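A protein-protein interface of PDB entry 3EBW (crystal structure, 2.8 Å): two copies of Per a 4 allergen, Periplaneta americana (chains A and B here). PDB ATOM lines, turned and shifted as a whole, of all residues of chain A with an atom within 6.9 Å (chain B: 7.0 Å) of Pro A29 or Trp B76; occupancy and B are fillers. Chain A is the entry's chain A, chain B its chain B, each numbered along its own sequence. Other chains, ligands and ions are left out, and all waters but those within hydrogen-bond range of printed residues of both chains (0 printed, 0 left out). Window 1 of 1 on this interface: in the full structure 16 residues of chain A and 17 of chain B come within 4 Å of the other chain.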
ATOM      1  N   ARG A  27      19.793 -20.080  31.839  1.00  0.00           N
ATOM      2  CA  ARG A  27      19.950 -18.792  32.495  1.00  0.00           C
ATOM      3  C   ARG A  27      19.862 -17.680  31.472  1.00  0.00           C
ATOM      4  O   ARG A  27      20.138 -17.892  30.292  1.00  0.00           O
ATOM      5  CB  ARG A  27      21.317 -18.691  33.170  1.00  0.00           C
ATOM      6  CG  ARG A  27      22.462 -18.600  32.163  1.00  0.00           C
ATOM      7  CD  ARG A  27      23.775 -18.146  32.760  1.00  0.00           C
ATOM      8  NE  ARG A  27      24.664 -19.266  33.063  1.00  0.00           N
ATOM      9  CZ  ARG A  27      25.922 -19.368  32.635  1.00  0.00           C
ATOM     10  NH1 ARG A  27      26.459 -18.419  31.877  1.00  0.00           N
ATOM     11  NH2 ARG A  27      26.643 -20.427  32.961  1.00  0.00           N
ATOM     12  N   THR A  28      19.477 -16.496  31.923  1.00  0.00           N
ATOM     13  CA  THR A  28      19.430 -15.344  31.051  1.00  0.00           C
ATOM     14  C   THR A  28      20.903 -15.055  30.831  1.00  0.00           C
ATOM     15  O   THR A  28      21.657 -14.951  31.798  1.00  0.00           O
ATOM     16  CB  THR A  28      18.798 -14.126  31.758  1.00  0.00           C
ATOM     17  OG1 THR A  28      17.375 -14.261  31.765  1.00  0.00           O
ATOM     18  CG2 THR A  28      19.202 -12.821  31.067  1.00  0.00           C
ATOM     19  N   PRO A  29      21.342 -14.946  29.569  1.00  0.00           N
ATOM     20  CA  PRO A  29      22.736 -14.665  29.205  1.00  0.00           C
ATOM     21  C   PRO A  29      23.155 -13.359  29.852  1.00  0.00           C
ATOM     22  O   PRO A  29      22.377 -12.424  29.869  1.00  0.00           O
ATOM     23  CB  PRO A  29      22.672 -14.516  27.691  1.00  0.00           C
ATOM     24  CG  PRO A  29      21.512 -15.346  27.303  1.00  0.00           C
ATOM     25  CD  PRO A  29      20.500 -15.051  28.370  1.00  0.00           C
ATOM     26  N   ASN A  30      24.368 -13.274  30.376  1.00  0.00           N
ATOM     27  CA  ASN A  30      24.825 -12.034  31.023  1.00  0.00           C
ATOM     28  C   ASN A  30      26.336 -12.092  31.206  1.00  0.00           C
ATOM     29  O   ASN A  30      26.907 -13.177  31.237  1.00  0.00           O
ATOM     30  CB  ASN A  30      24.185 -11.871  32.409  1.00  0.00           C
ATOM     31  CG  ASN A  30      24.663 -12.928  33.400  1.00  0.00           C
ATOM     32  OD1 ASN A  30      24.105 -14.017  33.499  1.00  0.00           O
ATOM     33  ND2 ASN A  30      25.722 -12.609  34.117  1.00  0.00           N
ATOM     34  N   SER A  31      26.968 -10.933  31.354  1.00  0.00           N
ATOM     35  CA  SER A  31      28.411 -10.850  31.509  1.00  0.00           C
ATOM     36  C   SER A  31      28.912 -11.635  32.712  1.00  0.00           C
ATOM     37  O   SER A  31      29.323 -12.780  32.564  1.00  0.00           O
ATOM     38  CB  SER A  31      28.837  -9.388  31.620  1.00  0.00           C
ATOM     39  OG  SER A  31      28.083  -8.722  32.614  1.00  0.00           O
ATOM     40  N   GLU A  33      29.081 -14.129  34.689  1.00  0.00           N
ATOM     41  CA  GLU A  33      28.493 -15.469  34.713  1.00  0.00           C
ATOM     42  C   GLU A  33      28.802 -16.129  33.354  1.00  0.00           C
ATOM     43  O   GLU A  33      28.426 -17.294  33.095  1.00  0.00           O
ATOM     44  CB  GLU A  33      26.978 -15.399  34.936  1.00  0.00           C
ATOM     45  CG  GLU A  33      26.270 -16.742  35.019  1.00  0.00           C
ATOM     46  CD  GLU A  33      24.965 -16.653  35.808  1.00  0.00           C
ATOM     47  OE1 GLU A  33      24.644 -15.527  36.232  1.00  0.00           O
ATOM     48  OE2 GLU A  33      24.267 -17.685  36.008  1.00  0.00           O
ATOM     49  N   GLU A  34      29.515 -15.362  32.517  1.00  0.00           N
ATOM     50  CA  GLU A  34      29.944 -15.725  31.160  1.00  0.00           C
ATOM     51  C   GLU A  34      30.788 -16.977  31.063  1.00  0.00           C
ATOM     52  O   GLU A  34      30.558 -17.818  30.182  1.00  0.00           O
ATOM     53  CB  GLU A  34      30.763 -14.588  30.562  1.00  0.00           C
ATOM     54  CG  GLU A  34      30.128 -13.849  29.418  1.00  0.00           C
ATOM     55  CD  GLU A  34      31.001 -12.713  28.962  1.00  0.00           C
ATOM     56  OE1 GLU A  34      32.004 -12.983  28.279  1.00  0.00           O
ATOM     57  OE2 GLU A  34      30.704 -11.551  29.302  1.00  0.00           O
ATOM     58  N   ARG A 118      18.032  -4.462  34.279  1.00  0.00           N
ATOM     59  CA  ARG A 118      18.196  -5.772  33.659  1.00  0.00           C
ATOM     60  C   ARG A 118      17.818  -6.945  34.576  1.00  0.00           C
ATOM     61  O   ARG A 118      18.486  -7.207  35.592  1.00  0.00           O
ATOM     62  CB  ARG A 118      19.655  -5.923  33.200  1.00  0.00           C
ATOM     63  CG  ARG A 118      19.878  -6.763  31.938  1.00  0.00           C
ATOM     64  CD  ARG A 118      19.532  -8.224  32.150  1.00  0.00           C
ATOM     65  NE  ARG A 118      19.692  -9.035  30.945  1.00  0.00           N
ATOM     66  CZ  ARG A 118      20.832  -9.170  30.288  1.00  0.00           C
ATOM     67  NH1 ARG A 118      21.914  -8.542  30.714  1.00  0.00           N
ATOM     68  NH2 ARG A 118      20.892  -9.954  29.222  1.00  0.00           N
ATOM     69  N   HIS A 119      16.757  -7.653  34.208  1.00  0.00           N
ATOM     70  CA  HIS A 119      16.328  -8.806  34.982  1.00  0.00           C
ATOM     71  C   HIS A 119      17.042 -10.071  34.528  1.00  0.00           C
ATOM     72  O   HIS A 119      17.391 -10.210  33.355  1.00  0.00           O
ATOM     73  CB  HIS A 119      14.822  -9.003  34.856  1.00  0.00           C
ATOM     74  CG  HIS A 119      14.022  -7.916  35.500  1.00  0.00           C
ATOM     75  ND1 HIS A 119      12.679  -8.044  35.773  1.00  0.00           N
ATOM     76  CD2 HIS A 119      14.388  -6.689  35.945  1.00  0.00           C
ATOM     77  CE1 HIS A 119      12.252  -6.943  36.366  1.00  0.00           C
ATOM     78  NE2 HIS A 119      13.268  -6.106  36.483  1.00  0.00           N
ATOM     79  N   LEU A 120      17.260 -11.002  35.450  1.00  0.00           N
ATOM     80  CA  LEU A 120      17.936 -12.246  35.105  1.00  0.00           C
ATOM     81  C   LEU A 120      17.118 -13.430  35.593  1.00  0.00           C
ATOM     82  O   LEU A 120      16.720 -13.465  36.757  1.00  0.00           O
ATOM     83  CB  LEU A 120      19.333 -12.305  35.755  1.00  0.00           C
ATOM     84  CG  LEU A 120      20.481 -11.323  35.449  1.00  0.00           C
ATOM     85  CD1 LEU A 120      20.842 -11.360  33.989  1.00  0.00           C
ATOM     86  CD2 LEU A 120      20.078  -9.935  35.804  1.00  0.00           C
ATOM     87  N   TYR A 121      16.849 -14.397  34.724  1.00  0.00           N
ATOM     88  CA  TYR A 121      16.113 -15.590  35.169  1.00  0.00           C
ATOM     89  C   TYR A 121      17.056 -16.780  35.210  1.00  0.00           C
ATOM     90  O   TYR A 121      17.918 -16.905  34.361  1.00  0.00           O
ATOM     91  CB  TYR A 121      14.924 -15.912  34.250  1.00  0.00           C
ATOM     92  CG  TYR A 121      13.821 -14.887  34.322  1.00  0.00           C
ATOM     93  CD1 TYR A 121      12.581 -15.210  34.869  1.00  0.00           C
ATOM     94  CD2 TYR A 121      14.029 -13.591  33.871  1.00  0.00           C
ATOM     95  CE1 TYR A 121      11.582 -14.279  34.962  1.00  0.00           C
ATOM     96  CE2 TYR A 121      13.043 -12.649  33.961  1.00  0.00           C
ATOM     97  CZ  TYR A 121      11.809 -12.995  34.506  1.00  0.00           C
ATOM     98  OH  TYR A 121      10.794 -12.066  34.551  1.00  0.00           O
ATOM     99  N   ASP A 151      14.788 -19.305  24.992  1.00  0.00           N
ATOM    100  CA  ASP A 151      14.961 -17.868  24.846  1.00  0.00           C
ATOM    101  C   ASP A 151      16.171 -17.494  25.697  1.00  0.00           C
ATOM    102  O   ASP A 151      16.583 -16.335  25.754  1.00  0.00           O
ATOM    103  CB  ASP A 151      13.697 -17.165  25.359  1.00  0.00           C
ATOM    104  CG  ASP A 151      13.368 -15.910  24.588  1.00  0.00           C
ATOM    105  OD1 ASP A 151      12.286 -15.343  24.839  1.00  0.00           O
ATOM    106  OD2 ASP A 151      14.183 -15.494  23.740  1.00  0.00           O
ATOM    107  N   MET A 152      16.732 -18.499  26.360  1.00  0.00           N
ATOM    108  CA  MET A 152      17.892 -18.295  27.207  1.00  0.00           C
ATOM    109  C   MET A 152      18.966 -19.372  27.083  1.00  0.00           C
ATOM    110  O   MET A 152      18.724 -20.465  26.578  1.00  0.00           O
ATOM    111  CB  MET A 152      17.443 -18.147  28.649  1.00  0.00           C
ATOM    112  CG  MET A 152      16.442 -19.160  29.067  1.00  0.00           C
ATOM    113  SD  MET A 152      15.421 -18.469  30.525  1.00  0.00           S
ATOM    114  CE  MET A 152      14.169 -19.943  30.646  1.00  0.00           C
ATOM    115  N   GLU A 153      20.150 -19.032  27.579  1.00  0.00           N
ATOM    116  CA  GLU A 153      21.354 -19.863  27.525  1.00  0.00           C
ATOM    117  C   GLU A 153      21.456 -21.124  28.402  1.00  0.00           C
ATOM    118  O   GLU A 153      21.502 -21.040  29.625  1.00  0.00           O
ATOM    119  CB  GLU A 153      22.553 -18.950  27.811  1.00  0.00           C
ATOM    120  CG  GLU A 153      23.914 -19.518  27.553  1.00  0.00           C
ATOM    121  CD  GLU A 153      24.999 -18.528  27.931  1.00  0.00           C
ATOM    122  OE1 GLU A 153      25.374 -18.452  29.119  1.00  0.00           O
ATOM    123  OE2 GLU A 153      25.478 -17.795  27.049  1.00  0.00           O
ATOM    124  N   GLY B  12      35.736 -11.263  26.777  1.00  0.00           N
ATOM    125  CA  GLY B  12      35.035 -10.353  27.659  1.00  0.00           C
ATOM    126  C   GLY B  12      33.816  -9.775  26.977  1.00  0.00           C
ATOM    127  O   GLY B  12      33.328  -8.718  27.368  1.00  0.00           O
ATOM    128  N   LEU B  13      33.326 -10.474  25.953  1.00  0.00           N
ATOM    129  CA  LEU B  13      32.165 -10.024  25.202  1.00  0.00           C
ATOM    130  C   LEU B  13      30.969  -9.880  26.132  1.00  0.00           C
ATOM    131  O   LEU B  13      30.666 -10.768  26.905  1.00  0.00           O
ATOM    132  CB  LEU B  13      31.847 -11.010  24.066  1.00  0.00           C
ATOM    133  CG  LEU B  13      30.575 -10.704  23.255  1.00  0.00           C
ATOM    134  CD1 LEU B  13      30.656  -9.319  22.618  1.00  0.00           C
ATOM    135  CD2 LEU B  13      30.374 -11.791  22.227  1.00  0.00           C
ATOM    136  N   ASP B  14      30.299  -8.743  26.050  1.00  0.00           N
ATOM    137  CA  ASP B  14      29.135  -8.464  26.879  1.00  0.00           C
ATOM    138  C   ASP B  14      28.018  -7.862  25.986  1.00  0.00           C
ATOM    139  O   ASP B  14      27.902  -6.638  25.830  1.00  0.00           O
ATOM    140  CB  ASP B  14      29.551  -7.504  28.006  1.00  0.00           C
ATOM    141  CG  ASP B  14      28.415  -7.169  28.949  1.00  0.00           C
ATOM    142  OD1 ASP B  14      27.388  -7.863  28.916  1.00  0.00           O
ATOM    143  OD2 ASP B  14      28.536  -6.211  29.741  1.00  0.00           O
ATOM    144  N   MET B  15      27.207  -8.748  25.402  1.00  0.00           N
ATOM    145  CA  MET B  15      26.124  -8.343  24.516  1.00  0.00           C
ATOM    146  C   MET B  15      25.204  -7.308  25.120  1.00  0.00           C
ATOM    147  O   MET B  15      24.348  -6.767  24.448  1.00  0.00           O
ATOM    148  CB  MET B  15      25.324  -9.562  24.047  1.00  0.00           C
ATOM    149  CG  MET B  15      26.098 -10.439  23.066  1.00  0.00           C
ATOM    150  SD  MET B  15      26.812  -9.426  21.554  1.00  0.00           S
ATOM    151  CE  MET B  15      25.240  -9.558  20.430  1.00  0.00           C
ATOM    152  N   THR B  16      25.391  -7.014  26.391  1.00  0.00           N
ATOM    153  CA  THR B  16      24.568  -6.018  27.031  1.00  0.00           C
ATOM    154  C   THR B  16      25.167  -4.664  26.691  1.00  0.00           C
ATOM    155  O   THR B  16      24.449  -3.684  26.552  1.00  0.00           O
ATOM    156  CB  THR B  16      24.552  -6.229  28.539  1.00  0.00           C
ATOM    157  OG1 THR B  16      24.387  -7.624  28.804  1.00  0.00           O
ATOM    158  CG2 THR B  16      23.387  -5.476  29.162  1.00  0.00           C
ATOM    159  N   LYS B  17      26.487  -4.620  26.552  1.00  0.00           N
ATOM    160  CA  LYS B  17      27.179  -3.389  26.195  1.00  0.00           C
ATOM    161  C   LYS B  17      27.116  -3.180  24.682  1.00  0.00           C
ATOM    162  O   LYS B  17      27.585  -2.170  24.160  1.00  0.00           O
ATOM    163  CB  LYS B  17      28.647  -3.458  26.622  1.00  0.00           C
ATOM    164  CG  LYS B  17      28.914  -3.256  28.106  1.00  0.00           C
ATOM    165  CD  LYS B  17      30.414  -3.323  28.364  1.00  0.00           C
ATOM    166  CE  LYS B  17      30.779  -3.061  29.803  1.00  0.00           C
ATOM    167  NZ  LYS B  17      32.217  -3.390  30.015  1.00  0.00           N
ATOM    168  N   GLY B  50      14.931  -9.490  30.575  1.00  0.00           N
ATOM    169  CA  GLY B  50      16.316  -9.831  30.330  1.00  0.00           C
ATOM    170  C   GLY B  50      16.712 -10.163  28.908  1.00  0.00           C
ATOM    171  O   GLY B  50      17.892 -10.147  28.602  1.00  0.00           O
ATOM    172  N   VAL B  51      15.744 -10.466  28.050  1.00  0.00           N
ATOM    173  CA  VAL B  51      16.038 -10.818  26.665  1.00  0.00           C
ATOM    174  C   VAL B  51      16.650  -9.706  25.839  1.00  0.00           C
ATOM    175  O   VAL B  51      16.169  -8.581  25.864  1.00  0.00           O
ATOM    176  CB  VAL B  51      14.777 -11.274  25.901  1.00  0.00           C
ATOM    177  CG1 VAL B  51      15.142 -11.559  24.457  1.00  0.00           C
ATOM    178  CG2 VAL B  51      14.188 -12.529  26.540  1.00  0.00           C
ATOM    179  N   ILE B  52      17.726 -10.012  25.120  1.00  0.00           N
ATOM    180  CA  ILE B  52      18.315  -9.011  24.245  1.00  0.00           C
ATOM    181  C   ILE B  52      17.665  -9.240  22.887  1.00  0.00           C
ATOM    182  O   ILE B  52      17.700 -10.333  22.310  1.00  0.00           O
ATOM    183  CB  ILE B  52      19.818  -9.131  24.107  1.00  0.00           C
ATOM    184  CG1 ILE B  52      20.478  -8.803  25.442  1.00  0.00           C
ATOM    185  CG2 ILE B  52      20.306  -8.154  23.029  1.00  0.00           C
ATOM    186  CD1 ILE B  52      21.956  -8.630  25.325  1.00  0.00           C
ATOM    187  N   VAL B  73      18.993 -12.626  20.968  1.00  0.00           N
ATOM    188  CA  VAL B  73      20.304 -13.260  21.118  1.00  0.00           C
ATOM    189  C   VAL B  73      20.223 -14.039  22.447  1.00  0.00           C
ATOM    190  O   VAL B  73      20.502 -13.515  23.495  1.00  0.00           O
ATOM    191  CB  VAL B  73      21.503 -12.217  21.074  1.00  0.00           C
ATOM    192  CG1 VAL B  73      21.016 -10.811  21.350  1.00  0.00           C
ATOM    193  CG2 VAL B  73      22.595 -12.630  22.061  1.00  0.00           C
ATOM    194  N   PRO B  74      19.820 -15.316  22.382  1.00  0.00           N
ATOM    195  CA  PRO B  74      19.639 -16.258  23.482  1.00  0.00           C
ATOM    196  C   PRO B  74      20.849 -16.689  24.270  1.00  0.00           C
ATOM    197  O   PRO B  74      20.707 -17.255  25.348  1.00  0.00           O
ATOM    198  CB  PRO B  74      18.939 -17.432  22.808  1.00  0.00           C
ATOM    199  CG  PRO B  74      19.613 -17.482  21.526  1.00  0.00           C
ATOM    200  CD  PRO B  74      19.642 -16.020  21.100  1.00  0.00           C
ATOM    201  N   SER B  75      22.039 -16.457  23.742  1.00  0.00           N
ATOM    202  CA  SER B  75      23.246 -16.823  24.478  1.00  0.00           C
ATOM    203  C   SER B  75      24.451 -16.131  23.908  1.00  0.00           C
ATOM    204  O   SER B  75      24.362 -15.433  22.915  1.00  0.00           O
ATOM    205  CB  SER B  75      23.467 -18.320  24.434  1.00  0.00           C
ATOM    206  OG  SER B  75      23.983 -18.701  23.198  1.00  0.00           O
ATOM    207  N   TRP B  76      25.580 -16.307  24.562  1.00  0.00           N
ATOM    208  CA  TRP B  76      26.809 -15.701  24.091  1.00  0.00           C
ATOM    209  C   TRP B  76      27.994 -16.071  24.959  1.00  0.00           C
ATOM    210  O   TRP B  76      27.946 -15.982  26.186  1.00  0.00           O
ATOM    211  CB  TRP B  76      26.653 -14.175  23.969  1.00  0.00           C
ATOM    212  CG  TRP B  76      26.832 -13.333  25.191  1.00  0.00           C
ATOM    213  CD1 TRP B  76      28.017 -12.975  25.782  1.00  0.00           C
ATOM    214  CD2 TRP B  76      25.810 -12.590  25.872  1.00  0.00           C
ATOM    215  NE1 TRP B  76      27.789 -12.037  26.774  1.00  0.00           N
ATOM    216  CE2 TRP B  76      26.446 -11.787  26.844  1.00  0.00           C
ATOM    217  CE3 TRP B  76      24.419 -12.514  25.744  1.00  0.00           C
ATOM    218  CZ2 TRP B  76      25.736 -10.926  27.670  1.00  0.00           C
ATOM    219  CZ3 TRP B  76      23.723 -11.655  26.566  1.00  0.00           C
ATOM    220  CH2 TRP B  76      24.379 -10.872  27.513  1.00  0.00           C
ATOM    221  N   THR B  77      29.050 -16.529  24.305  1.00  0.00           N
ATOM    222  CA  THR B  77      30.270 -16.927  24.974  1.00  0.00           C
ATOM    223  C   THR B  77      31.234 -15.776  25.154  1.00  0.00           C
ATOM    224  O   THR B  77      30.849 -14.615  25.089  1.00  0.00           O
ATOM    225  CB  THR B  77      30.953 -18.024  24.209  1.00  0.00           C
ATOM    226  OG1 THR B  77      29.954 -18.918  23.727  1.00  0.00           O
ATOM    227  CG2 THR B  77      31.890 -18.808  25.132  1.00  0.00           C
ATOM    228  N   GLU B  78      32.493 -16.111  25.402  1.00  0.00           N
ATOM    229  CA  GLU B  78      33.543 -15.134  25.633  1.00  0.00           C
ATOM    230  C   GLU B  78      33.764 -14.210  24.426  1.00  0.00           C
ATOM    231  O   GLU B  78      34.107 -13.042  24.588  1.00  0.00           O
ATOM    232  CB  GLU B  78      34.824 -15.878  26.013  1.00  0.00           C
ATOM    233  CG  GLU B  78      35.754 -15.083  26.906  1.00  0.00           C
ATOM    234  CD  GLU B  78      35.047 -14.511  28.112  1.00  0.00           C
ATOM    235  OE1 GLU B  78      34.614 -15.297  28.981  1.00  0.00           O
ATOM    236  OE2 GLU B  78      34.922 -13.269  28.186  1.00  0.00           O
ATOM    237  N   ASP B  79      33.538 -14.732  23.223  1.00  0.00           N
ATOM    238  CA  ASP B  79      33.690 -13.947  21.987  1.00  0.00           C
ATOM    239  C   ASP B  79      32.775 -14.526  20.895  1.00  0.00           C
ATOM    240  O   ASP B  79      33.160 -14.619  19.731  1.00  0.00           O
ATOM    241  CB  ASP B  79      35.131 -14.013  21.511  1.00  0.00           C
ATOM    242  CG  ASP B  79      35.544 -15.423  21.096  1.00  0.00           C
ATOM    243  OD1 ASP B  79      34.745 -16.374  21.268  1.00  0.00           O
ATOM    244  OD2 ASP B  79      36.678 -15.579  20.592  1.00  0.00           O
ATOM    245  N   THR B  80      31.565 -14.912  21.283  1.00  0.00           N
ATOM    246  CA  THR B  80      30.623 -15.518  20.360  1.00  0.00           C
ATOM    247  C   THR B  80      29.214 -15.149  20.740  1.00  0.00           C
ATOM    248  O   THR B  80      28.941 -14.949  21.903  1.00  0.00           O
ATOM    249  CB  THR B  80      30.771 -17.050  20.423  1.00  0.00           C
ATOM    250  OG1 THR B  80      31.774 -17.457  19.489  1.00  0.00           O
ATOM    251  CG2 THR B  80      29.454 -17.762  20.151  1.00  0.00           C
ATOM    252  N   PHE B  81      28.318 -15.000  19.773  1.00  0.00           N
ATOM    253  CA  PHE B  81      26.936 -14.739  20.151  1.00  0.00           C
ATOM    254  C   PHE B  81      26.003 -15.435  19.196  1.00  0.00           C
ATOM    255  O   PHE B  81      26.318 -15.586  18.031  1.00  0.00           O
ATOM    256  CB  PHE B  81      26.623 -13.239  20.268  1.00  0.00           C
ATOM    257  CG  PHE B  81      26.751 -12.469  18.997  1.00  0.00           C
ATOM    258  CD1 PHE B  81      27.961 -11.886  18.645  1.00  0.00           C
ATOM    259  CD2 PHE B  81      25.637 -12.245  18.190  1.00  0.00           C
ATOM    260  CE1 PHE B  81      28.053 -11.093  17.511  1.00  0.00           C
ATOM    261  CE2 PHE B  81      25.723 -11.457  17.058  1.00  0.00           C
ATOM    262  CZ  PHE B  81      26.927 -10.879  16.719  1.00  0.00           C
ATOM    263  N   ASP B  82      24.875 -15.918  19.693  1.00  0.00           N
ATOM    264  CA  ASP B  82      23.943 -16.607  18.825  1.00  0.00           C
ATOM    265  C   ASP B  82      22.685 -15.764  18.584  1.00  0.00           C
ATOM    266  O   ASP B  82      22.368 -14.853  19.358  1.00  0.00           O
ATOM    267  CB  ASP B  82      23.582 -17.971  19.421  1.00  0.00           C
ATOM    268  CG  ASP B  82      24.833 -18.855  19.715  1.00  0.00           C
ATOM    269  OD1 ASP B  82      24.713 -20.110  19.650  1.00  0.00           O
ATOM    270  OD2 ASP B  82      25.933 -18.305  20.028  1.00  0.00           O
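O of Gly B50 touches CG2 of Thr A28 (3.9 Å).
Pro A29 touches Pro B74.
Pro A29 touches Ser B75 (CG to CA, 3.6 Å).
Pro A29 touches Trp B76 (CB to CZ3, 3.2 Å).
Asn A30 touches Trp B76.
Ser A31 touches Asp B14 (CB to OD1, 3.4 Å).
Trp B76 touches Ser A31.
Gly B12 touches Glu A34 (C to OE1, 3.9 Å).
Arg A118 touches Trp B76 (NH2 to CH2, 3.99 Å).
Glu A153 touches Ser B75 (OE2 to CB, 3.3 Å).
Of the 19 printed residues of chain B, 12 touch a printed residue of chain A.
Hydrophobic or aromatic side chains of chain B that line the printed part of chain A: Val B51, Ile B52, Pro B74 and Trp B76.
Hydrophobic or aromatic side chains of chain A that line the printed part of chain B: Pro A29.
Among the printed residues, no Asp or Glu carboxylate lies within 4 Å of a Lys or Arg side-chain nitrogen of the other chain.
Pro A29 touches just these residues of chain B: Pro B74, Ser B75 and Trp B76.
Printed residues of chain A within 4 Å of Asp B14: Ser A31 (3.4 Å).
Of the printed residues of chain A, Gly B50 touches Thr A28, Arg A118 and His A119.
Of the printed residues of chain A, Trp B76 touches Pro A29, Asn A30, Ser A31, Glu A34, Arg A118 and Glu A153.
Of the printed residues of chain A, Glu B78 touches Glu A34.
Phe B81 touches none of the printed residues of chain A.
The nearest printed residue of chain A that does not touch Gly B50 is Tyr A121 (5.0 Å).
The side-chain carboxylate (OE1) of Glu A34 sits close to the side-chain carboxylate (OE2) of Glu B78 (2.9 Å).
OE2 of Glu A34 sits close to O of Leu B13 (2.5 Å).
The side-chain carboxylate of Glu A153 lies within hydrogen-bond range of the backbone NH of Trp B76 (2.9 Å).
O of Pro B74 sits at hydrogen-bond distance from N of Glu A153, at 2.9 Å.
The guanidinium group of Arg A118 is in hydrogen-bond range of the backbone carbonyl oxygen of Gly B50, at 3.1 Å.
The guanidinium group (NH1) of Arg A118 is in hydrogen-bond range of the side-chain hydroxyl (OG1) of Thr B16 (3.3 Å).
No position is printed for both chains.
O of Tyr A121 lies within hydrogen-bond range of N of Thr A28 (2.9 Å).
The side-chain carboxylate (OE1) of Glu A33 lies close to the side-chain amide oxygen (OD1) of Asn A30, 3.2 Å away.
N of Gly B12 lies within hydrogen-bond range of OE2 of Glu B78.
The guanidinium group of Arg A27 is in salt-bridge range of the side-chain carboxylate of Glu A153 (3.0 Å).
OD1 of Asn A30 sits close to O of Thr A28 (3.1 Å).
The backbone carbonyl oxygen of Glu B78 sits at hydrogen-bond distance from the backbone NH of Leu B13, 3.0 Å away.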
